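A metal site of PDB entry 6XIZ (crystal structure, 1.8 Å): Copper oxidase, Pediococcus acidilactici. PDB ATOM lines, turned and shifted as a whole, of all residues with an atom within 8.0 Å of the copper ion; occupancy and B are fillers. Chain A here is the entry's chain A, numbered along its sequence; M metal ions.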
ATOM      1  N   VAL A 208      27.812  19.890 -16.997  1.00  0.00           N
ATOM      2  CA  VAL A 208      26.785  20.595 -17.687  1.00  0.00           C
ATOM      3  C   VAL A 208      26.412  19.943 -19.015  1.00  0.00           C
ATOM      4  O   VAL A 208      25.286  20.103 -19.482  1.00  0.00           O
ATOM      5  CB  VAL A 208      27.213  22.070 -17.933  1.00  0.00           C
ATOM      6  CG1 VAL A 208      28.465  22.115 -18.861  1.00  0.00           C
ATOM      7  CG2 VAL A 208      25.996  22.926 -18.434  1.00  0.00           C
ATOM      8  N   ASP A 209      27.340  19.148 -19.561  1.00  0.00           N
ATOM      9  CA  ASP A 209      27.057  18.396 -20.797  1.00  0.00           C
ATOM     10  C   ASP A 209      26.389  17.019 -20.594  1.00  0.00           C
ATOM     11  O   ASP A 209      26.039  16.352 -21.609  1.00  0.00           O
ATOM     12  CB  ASP A 209      28.333  18.226 -21.605  1.00  0.00           C
ATOM     13  CG  ASP A 209      28.011  17.992 -23.111  1.00  0.00           C
ATOM     14  OD1 ASP A 209      26.908  18.538 -23.561  1.00  0.00           O
ATOM     15  OD2 ASP A 209      28.802  17.265 -23.787  1.00  0.00           O
ATOM     16  N   ARG A 243      22.547  10.981 -18.827  1.00  0.00           N
ATOM     17  CA  ARG A 243      23.269  11.239 -20.138  1.00  0.00           C
ATOM     18  C   ARG A 243      23.703   9.973 -20.832  1.00  0.00           C
ATOM     19  O   ARG A 243      23.601   9.921 -22.054  1.00  0.00           O
ATOM     20  CB  ARG A 243      24.436  12.148 -19.955  1.00  0.00           C
ATOM     21  CG  ARG A 243      25.652  11.969 -20.953  1.00  0.00           C
ATOM     22  CD  ARG A 243      25.563  12.790 -22.032  1.00  0.00           C
ATOM     23  NE  ARG A 243      26.370  12.523 -23.283  1.00  0.00           N
ATOM     24  CZ  ARG A 243      25.947  11.914 -24.341  1.00  0.00           C
ATOM     25  NH1 ARG A 243      24.925  11.095 -24.308  1.00  0.00           N
ATOM     26  NH2 ARG A 243      26.604  12.077 -25.482  1.00  0.00           N
ATOM     27  N   MET A 345      17.630  21.801 -32.468  1.00  0.00           N
ATOM     28  CA  MET A 345      18.506  21.627 -31.312  1.00  0.00           C
ATOM     29  C   MET A 345      19.935  21.981 -31.751  1.00  0.00           C
ATOM     30  O   MET A 345      20.392  21.526 -32.825  1.00  0.00           O
ATOM     31  CB  MET A 345      18.440  20.129 -30.873  1.00  0.00           C
ATOM     32  CG  MET A 345      17.011  19.555 -30.556  1.00  0.00           C
ATOM     33  SD  MET A 345      17.095  17.826 -29.952  1.00  0.00           S
ATOM     34  CE  MET A 345      17.512  18.234 -28.363  1.00  0.00           C
ATOM     35  N   SER A 346      20.640  22.742 -30.952  1.00  0.00           N
ATOM     36  CA  SER A 346      21.944  23.212 -31.369  1.00  0.00           C
ATOM     37  C   SER A 346      22.740  23.376 -30.098  1.00  0.00           C
ATOM     38  O   SER A 346      22.178  23.410 -29.008  1.00  0.00           O
ATOM     39  CB  SER A 346      21.816  24.562 -32.094  1.00  0.00           C
ATOM     40  OG  SER A 346      21.441  25.600 -31.147  1.00  0.00           O
ATOM     41  N   GLY A 347      24.033  23.328 -30.256  1.00  0.00           N
ATOM     42  CA  GLY A 347      24.946  23.478 -29.177  1.00  0.00           C
ATOM     43  C   GLY A 347      25.140  22.212 -28.349  1.00  0.00           C
ATOM     44  O   GLY A 347      24.499  21.161 -28.577  1.00  0.00           O
ATOM     45  N   MET A 348      26.078  22.342 -27.396  1.00  0.00           N
ATOM     46  CA  MET A 348      26.540  21.338 -26.465  1.00  0.00           C
ATOM     47  C   MET A 348      26.928  22.085 -25.220  1.00  0.00           C
ATOM     48  O   MET A 348      27.058  23.304 -25.245  1.00  0.00           O
ATOM     49  CB  MET A 348      27.775  20.560 -26.995  1.00  0.00           C
ATOM     50  CG  MET A 348      27.418  19.780 -28.268  1.00  0.00           C
ATOM     51  SD  MET A 348      28.665  18.609 -28.925  1.00  0.00           S
ATOM     52  CE  MET A 348      29.927  19.891 -29.165  1.00  0.00           C
ATOM     53  N   ASP A 349      27.125  21.344 -24.136  1.00  0.00           N
ATOM     54  CA  ASP A 349      27.576  21.925 -22.879  1.00  0.00           C
ATOM     55  C   ASP A 349      26.586  23.055 -22.490  1.00  0.00           C
ATOM     56  O   ASP A 349      25.337  22.856 -22.593  1.00  0.00           O
ATOM     57  CB  ASP A 349      29.052  22.376 -23.020  1.00  0.00           C
ATOM     58  CG  ASP A 349      29.975  21.228 -23.563  1.00  0.00           C
ATOM     59  OD1 ASP A 349      30.219  20.268 -22.805  1.00  0.00           O
ATOM     60  OD2 ASP A 349      30.406  21.252 -24.748  1.00  0.00           O
ATOM     61  N   VAL A 352      23.839  24.868 -25.203  1.00  0.00           N
ATOM     62  CA  VAL A 352      22.695  24.172 -25.745  1.00  0.00           C
ATOM     63  C   VAL A 352      21.552  25.169 -25.945  1.00  0.00           C
ATOM     64  O   VAL A 352      21.317  25.978 -25.070  1.00  0.00           O
ATOM     65  CB  VAL A 352      22.156  22.960 -24.903  1.00  0.00           C
ATOM     66  CG1 VAL A 352      23.127  21.748 -24.978  1.00  0.00           C
ATOM     67  CG2 VAL A 352      21.920  23.322 -23.478  1.00  0.00           C
ATOM     68  N   ARG A 353      20.848  25.057 -27.083  1.00  0.00           N
ATOM     69  CA  ARG A 353      19.630  25.877 -27.309  1.00  0.00           C
ATOM     70  C   ARG A 353      18.541  25.107 -28.066  1.00  0.00           C
ATOM     71  O   ARG A 353      18.834  24.151 -28.845  1.00  0.00           O
ATOM     72  CB  ARG A 353      19.967  27.191 -28.052  1.00  0.00           C
ATOM     73  CG  ARG A 353      21.011  28.095 -27.431  1.00  0.00           C
ATOM     74  CD  ARG A 353      20.574  29.155 -26.433  1.00  0.00           C
ATOM     75  NE  ARG A 353      21.218  28.631 -25.298  1.00  0.00           N
ATOM     76  CZ  ARG A 353      22.252  29.127 -24.641  1.00  0.00           C
ATOM     77  NH1 ARG A 353      22.730  30.302 -24.825  1.00  0.00           N
ATOM     78  NH2 ARG A 353      22.692  28.421 -23.675  1.00  0.00           N
ATOM     79  N   ASN A 380      19.254  18.406 -35.471  1.00  0.00           N
ATOM     80  CA  ASN A 380      20.389  18.676 -34.590  1.00  0.00           C
ATOM     81  C   ASN A 380      21.555  19.230 -35.474  1.00  0.00           C
ATOM     82  O   ASN A 380      22.058  18.572 -36.412  1.00  0.00           O
ATOM     83  CB  ASN A 380      20.838  17.349 -33.976  1.00  0.00           C
ATOM     84  CG  ASN A 380      22.115  17.402 -33.226  1.00  0.00           C
ATOM     85  OD1 ASN A 380      22.783  18.366 -33.090  1.00  0.00           O
ATOM     86  ND2 ASN A 380      22.435  16.218 -32.615  1.00  0.00           N
ATOM     87  N   ASN A 382      24.689  20.041 -34.425  1.00  0.00           N
ATOM     88  CA  ASN A 382      26.024  19.765 -33.993  1.00  0.00           C
ATOM     89  C   ASN A 382      26.825  19.194 -35.186  1.00  0.00           C
ATOM     90  O   ASN A 382      26.234  18.525 -36.098  1.00  0.00           O
ATOM     91  CB  ASN A 382      26.079  18.727 -32.879  1.00  0.00           C
ATOM     92  CG  ASN A 382      25.507  19.223 -31.563  1.00  0.00           C
ATOM     93  OD1 ASN A 382      25.108  20.386 -31.366  1.00  0.00           O
ATOM     94  ND2 ASN A 382      25.403  18.331 -30.683  1.00  0.00           N
ATOM     95  N   MET A 388      27.037  15.314 -30.593  1.00  0.00           N
ATOM     96  CA  MET A 388      26.452  14.372 -29.707  1.00  0.00           C
ATOM     97  C   MET A 388      25.029  14.093 -30.154  1.00  0.00           C
ATOM     98  O   MET A 388      24.473  14.841 -30.994  1.00  0.00           O
ATOM     99  CB  MET A 388      26.586  14.890 -28.272  1.00  0.00           C
ATOM    100  CG  MET A 388      25.580  16.002 -27.927  1.00  0.00           C
ATOM    101  SD  MET A 388      26.136  16.923 -26.513  1.00  0.00           S
ATOM    102  CE  MET A 388      26.070  15.784 -25.151  1.00  0.00           C
ATOM    103  N   ILE A 389      24.466  12.968 -29.688  1.00  0.00           N
ATOM    104  CA  ILE A 389      23.102  12.560 -30.028  1.00  0.00           C
ATOM    105  C   ILE A 389      22.235  13.108 -28.942  1.00  0.00           C
ATOM    106  O   ILE A 389      22.420  12.841 -27.808  1.00  0.00           O
ATOM    107  CB  ILE A 389      23.010  11.057 -30.063  1.00  0.00           C
ATOM    108  CG1 ILE A 389      23.949  10.589 -31.138  1.00  0.00           C
ATOM    109  CG2 ILE A 389      21.568  10.645 -30.383  1.00  0.00           C
ATOM    110  CD1 ILE A 389      24.266   9.054 -31.091  1.00  0.00           C
ATOM    111  N   HIS A 390      21.304  13.971 -29.327  1.00  0.00           N
ATOM    112  CA  HIS A 390      20.353  14.559 -28.354  1.00  0.00           C
ATOM    113  C   HIS A 390      19.020  13.829 -28.357  1.00  0.00           C
ATOM    114  O   HIS A 390      18.399  13.685 -29.476  1.00  0.00           O
ATOM    115  CB  HIS A 390      20.019  16.003 -28.596  1.00  0.00           C
ATOM    116  CG  HIS A 390      21.181  16.869 -28.537  1.00  0.00           C
ATOM    117  ND1 HIS A 390      21.518  17.530 -27.394  1.00  0.00           N
ATOM    118  CD2 HIS A 390      22.133  17.191 -29.446  1.00  0.00           C
ATOM    119  CE1 HIS A 390      22.583  18.302 -27.610  1.00  0.00           C
ATOM    120  NE2 HIS A 390      22.973  18.125 -28.842  1.00  0.00           N
ATOM    121  N   PRO A 391      18.634  13.230 -27.199  1.00  0.00           N
ATOM    122  CA  PRO A 391      17.326  12.543 -27.200  1.00  0.00           C
ATOM    123  C   PRO A 391      16.138  13.558 -27.053  1.00  0.00           C
ATOM    124  O   PRO A 391      15.906  14.073 -26.040  1.00  0.00           O
ATOM    125  CB  PRO A 391      17.432  11.515 -26.052  1.00  0.00           C
ATOM    126  CG  PRO A 391      18.357  12.177 -25.088  1.00  0.00           C
ATOM    127  CD  PRO A 391      19.311  13.121 -25.922  1.00  0.00           C
ATOM    128  N   PHE A 392      15.369  13.648 -28.106  1.00  0.00           N
ATOM    129  CA  PHE A 392      14.263  14.572 -28.134  1.00  0.00           C
ATOM    130  C   PHE A 392      12.948  13.985 -27.639  1.00  0.00           C
ATOM    131  O   PHE A 392      12.479  12.994 -28.152  1.00  0.00           O
ATOM    132  CB  PHE A 392      14.118  15.065 -29.536  1.00  0.00           C
ATOM    133  CG  PHE A 392      13.020  16.093 -29.699  1.00  0.00           C
ATOM    134  CD1 PHE A 392      13.288  17.403 -29.449  1.00  0.00           C
ATOM    135  CD2 PHE A 392      11.755  15.695 -30.209  1.00  0.00           C
ATOM    136  CE1 PHE A 392      12.286  18.388 -29.634  1.00  0.00           C
ATOM    137  CE2 PHE A 392      10.760  16.681 -30.417  1.00  0.00           C
ATOM    138  CZ  PHE A 392      11.030  17.998 -30.081  1.00  0.00           C
ATOM    139  N   HIS A 443      11.599  18.844 -25.250  1.00  0.00           N
ATOM    140  CA  HIS A 443      12.931  19.142 -24.838  1.00  0.00           C
ATOM    141  C   HIS A 443      13.882  17.958 -25.054  1.00  0.00           C
ATOM    142  O   HIS A 443      13.498  16.870 -25.498  1.00  0.00           O
ATOM    143  CB  HIS A 443      12.996  19.452 -23.356  1.00  0.00           C
ATOM    144  CG  HIS A 443      12.429  18.399 -22.503  1.00  0.00           C
ATOM    145  ND1 HIS A 443      13.220  17.455 -21.883  1.00  0.00           N
ATOM    146  CD2 HIS A 443      11.162  18.103 -22.169  1.00  0.00           C
ATOM    147  CE1 HIS A 443      12.496  16.639 -21.184  1.00  0.00           C
ATOM    148  NE2 HIS A 443      11.238  17.018 -21.330  1.00  0.00           N
ATOM    149  N   CYS A 444      15.129  18.277 -24.897  1.00  0.00           N
ATOM    150  CA  CYS A 444      16.192  17.268 -24.798  1.00  0.00           C
ATOM    151  C   CYS A 444      16.101  16.544 -23.479  1.00  0.00           C
ATOM    152  O   CYS A 444      15.948  17.150 -22.475  1.00  0.00           O
ATOM    153  CB  CYS A 444      17.615  17.919 -24.970  1.00  0.00           C
ATOM    154  SG  CYS A 444      18.891  16.680 -24.875  1.00  0.00           S
ATOM    155  N   HIS A 445      16.281  15.227 -23.539  1.00  0.00           N
ATOM    156  CA  HIS A 445      16.214  14.453 -22.298  1.00  0.00           C
ATOM    157  C   HIS A 445      17.540  14.061 -21.655  1.00  0.00           C
ATOM    158  O   HIS A 445      17.609  13.274 -20.745  1.00  0.00           O
ATOM    159  CB  HIS A 445      15.278  13.215 -22.478  1.00  0.00           C
ATOM    160  CG  HIS A 445      14.544  12.829 -21.226  1.00  0.00           C
ATOM    161  ND1 HIS A 445      15.185  12.279 -20.124  1.00  0.00           N
ATOM    162  CD2 HIS A 445      13.231  12.885 -20.924  1.00  0.00           C
ATOM    163  CE1 HIS A 445      14.312  12.042 -19.194  1.00  0.00           C
ATOM    164  NE2 HIS A 445      13.138  12.447 -19.633  1.00  0.00           N
ATOM    165  N   ILE A 446      18.636  14.667 -22.125  1.00  0.00           N
ATOM    166  CA  ILE A 446      19.801  14.733 -21.339  1.00  0.00           C
ATOM    167  C   ILE A 446      19.516  15.732 -20.205  1.00  0.00           C
ATOM    168  O   ILE A 446      19.282  16.897 -20.527  1.00  0.00           O
ATOM    169  CB  ILE A 446      21.044  15.119 -22.131  1.00  0.00           C
ATOM    170  CG1 ILE A 446      21.360  13.976 -23.069  1.00  0.00           C
ATOM    171  CG2 ILE A 446      22.139  15.407 -21.175  1.00  0.00           C
ATOM    172  CD1 ILE A 446      22.271  14.335 -24.189  1.00  0.00           C
ATOM    173  N   LEU A 447      19.456  15.258 -18.958  1.00  0.00           N
ATOM    174  CA  LEU A 447      18.840  15.986 -17.844  1.00  0.00           C
ATOM    175  C   LEU A 447      19.567  17.272 -17.612  1.00  0.00           C
ATOM    176  O   LEU A 447      18.912  18.285 -17.434  1.00  0.00           O
ATOM    177  CB  LEU A 447      18.679  15.125 -16.560  1.00  0.00           C
ATOM    178  CG  LEU A 447      17.824  13.843 -16.796  1.00  0.00           C
ATOM    179  CD1 LEU A 447      17.648  13.046 -15.499  1.00  0.00           C
ATOM    180  CD2 LEU A 447      16.486  14.040 -17.465  1.00  0.00           C
ATOM    181  N   GLU A 448      20.888  17.278 -17.745  1.00  0.00           N
ATOM    182  CA  GLU A 448      21.589  18.523 -17.597  1.00  0.00           C
ATOM    183  C   GLU A 448      21.333  19.538 -18.717  1.00  0.00           C
ATOM    184  O   GLU A 448      21.366  20.767 -18.527  1.00  0.00           O
ATOM    185  CB  GLU A 448      23.065  18.266 -17.475  1.00  0.00           C
ATOM    186  CG  GLU A 448      23.391  17.736 -16.121  1.00  0.00           C
ATOM    187  CD  GLU A 448      23.165  16.230 -15.974  1.00  0.00           C
ATOM    188  OE1 GLU A 448      23.197  15.849 -14.799  1.00  0.00           O
ATOM    189  OE2 GLU A 448      22.898  15.470 -16.983  1.00  0.00           O
ATOM    190  N   HIS A 449      21.018  19.033 -19.890  1.00  0.00           N
ATOM    191  CA  HIS A 449      20.660  19.947 -21.001  1.00  0.00           C
ATOM    192  C   HIS A 449      19.288  20.593 -20.795  1.00  0.00           C
ATOM    193  O   HIS A 449      19.100  21.787 -21.113  1.00  0.00           O
ATOM    194  CB  HIS A 449      20.593  19.227 -22.306  1.00  0.00           C
ATOM    195  CG  HIS A 449      21.930  18.779 -22.816  1.00  0.00           C
ATOM    196  ND1 HIS A 449      22.067  18.257 -24.077  1.00  0.00           N
ATOM    197  CD2 HIS A 449      23.197  18.972 -22.338  1.00  0.00           C
ATOM    198  CE1 HIS A 449      23.363  17.929 -24.254  1.00  0.00           C
ATOM    199  NE2 HIS A 449      24.074  18.439 -23.274  1.00  0.00           N
ATOM    200  N   GLU A 450      18.355  19.759 -20.322  1.00  0.00           N
ATOM    201  CA  GLU A 450      17.004  20.157 -19.900  1.00  0.00           C
ATOM    202  C   GLU A 450      17.123  21.219 -18.842  1.00  0.00           C
ATOM    203  O   GLU A 450      16.527  22.299 -19.000  1.00  0.00           O
ATOM    204  CB  GLU A 450      16.259  18.906 -19.370  1.00  0.00           C
ATOM    205  CG  GLU A 450      14.850  19.146 -19.045  1.00  0.00           C
ATOM    206  CD  GLU A 450      14.299  17.969 -18.281  1.00  0.00           C
ATOM    207  OE1 GLU A 450      13.772  18.206 -17.184  1.00  0.00           O
ATOM    208  OE2 GLU A 450      14.470  16.823 -18.759  1.00  0.00           O
ATOM    209  N   MET A 454      17.222  23.637 -22.495  1.00  0.00           N
ATOM    210  CA  MET A 454      17.068  23.120 -23.791  1.00  0.00           C
ATOM    211  C   MET A 454      15.677  22.541 -23.821  1.00  0.00           C
ATOM    212  O   MET A 454      15.506  21.339 -23.936  1.00  0.00           O
ATOM    213  CB  MET A 454      18.217  22.083 -24.109  1.00  0.00           C
ATOM    214  CG  MET A 454      18.359  21.867 -25.606  1.00  0.00           C
ATOM    215  SD  MET A 454      19.567  20.570 -26.027  1.00  0.00           S
ATOM    216  CE  MET A 454      19.915  20.966 -27.719  1.00  0.00           C
HETATM  217 CU    CU M   1      20.741  17.683 -25.510  1.00  0.00          CU
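Ile 446 touches the copper ion (CD1 to CU, 3.9 Å). Met 454 touches the copper ion (SD to CU, 3.2 Å).
The copper ion is bound by a ring nitrogen (ND1) of His 449 (2.0 Å), a ring nitrogen (ND1) of His 390 (2.0 Å) and the side-chain sulfur (SG) of Cys 444 (2.2 Å). The copper ion has three donor atoms within binding distance.
The backbone carbonyl oxygen (O) of His 449 is in hydrogen-bond range of the backbone NH (N) of Met 454 (3.0 Å). NE2 of His 449 sits at hydrogen-bond distance from OD1 of Asp 209 (2.9 Å). A ring nitrogen (NE2) of His 390 sits at hydrogen-bond distance from the backbone carbonyl oxygen of Gly 347, at 3.4 Å. NE2 of His 390 sits at hydrogen-bond distance from ND2 of Asn 382 (3.1 Å). The side-chain sulfur of Cys 444 sits close to the backbone NH of Ile 446, at 3.4 Å. The backbone NH (N) of Cys 444 sits at hydrogen-bond distance from the backbone carbonyl oxygen (O) of Met 454 (3.2 Å).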
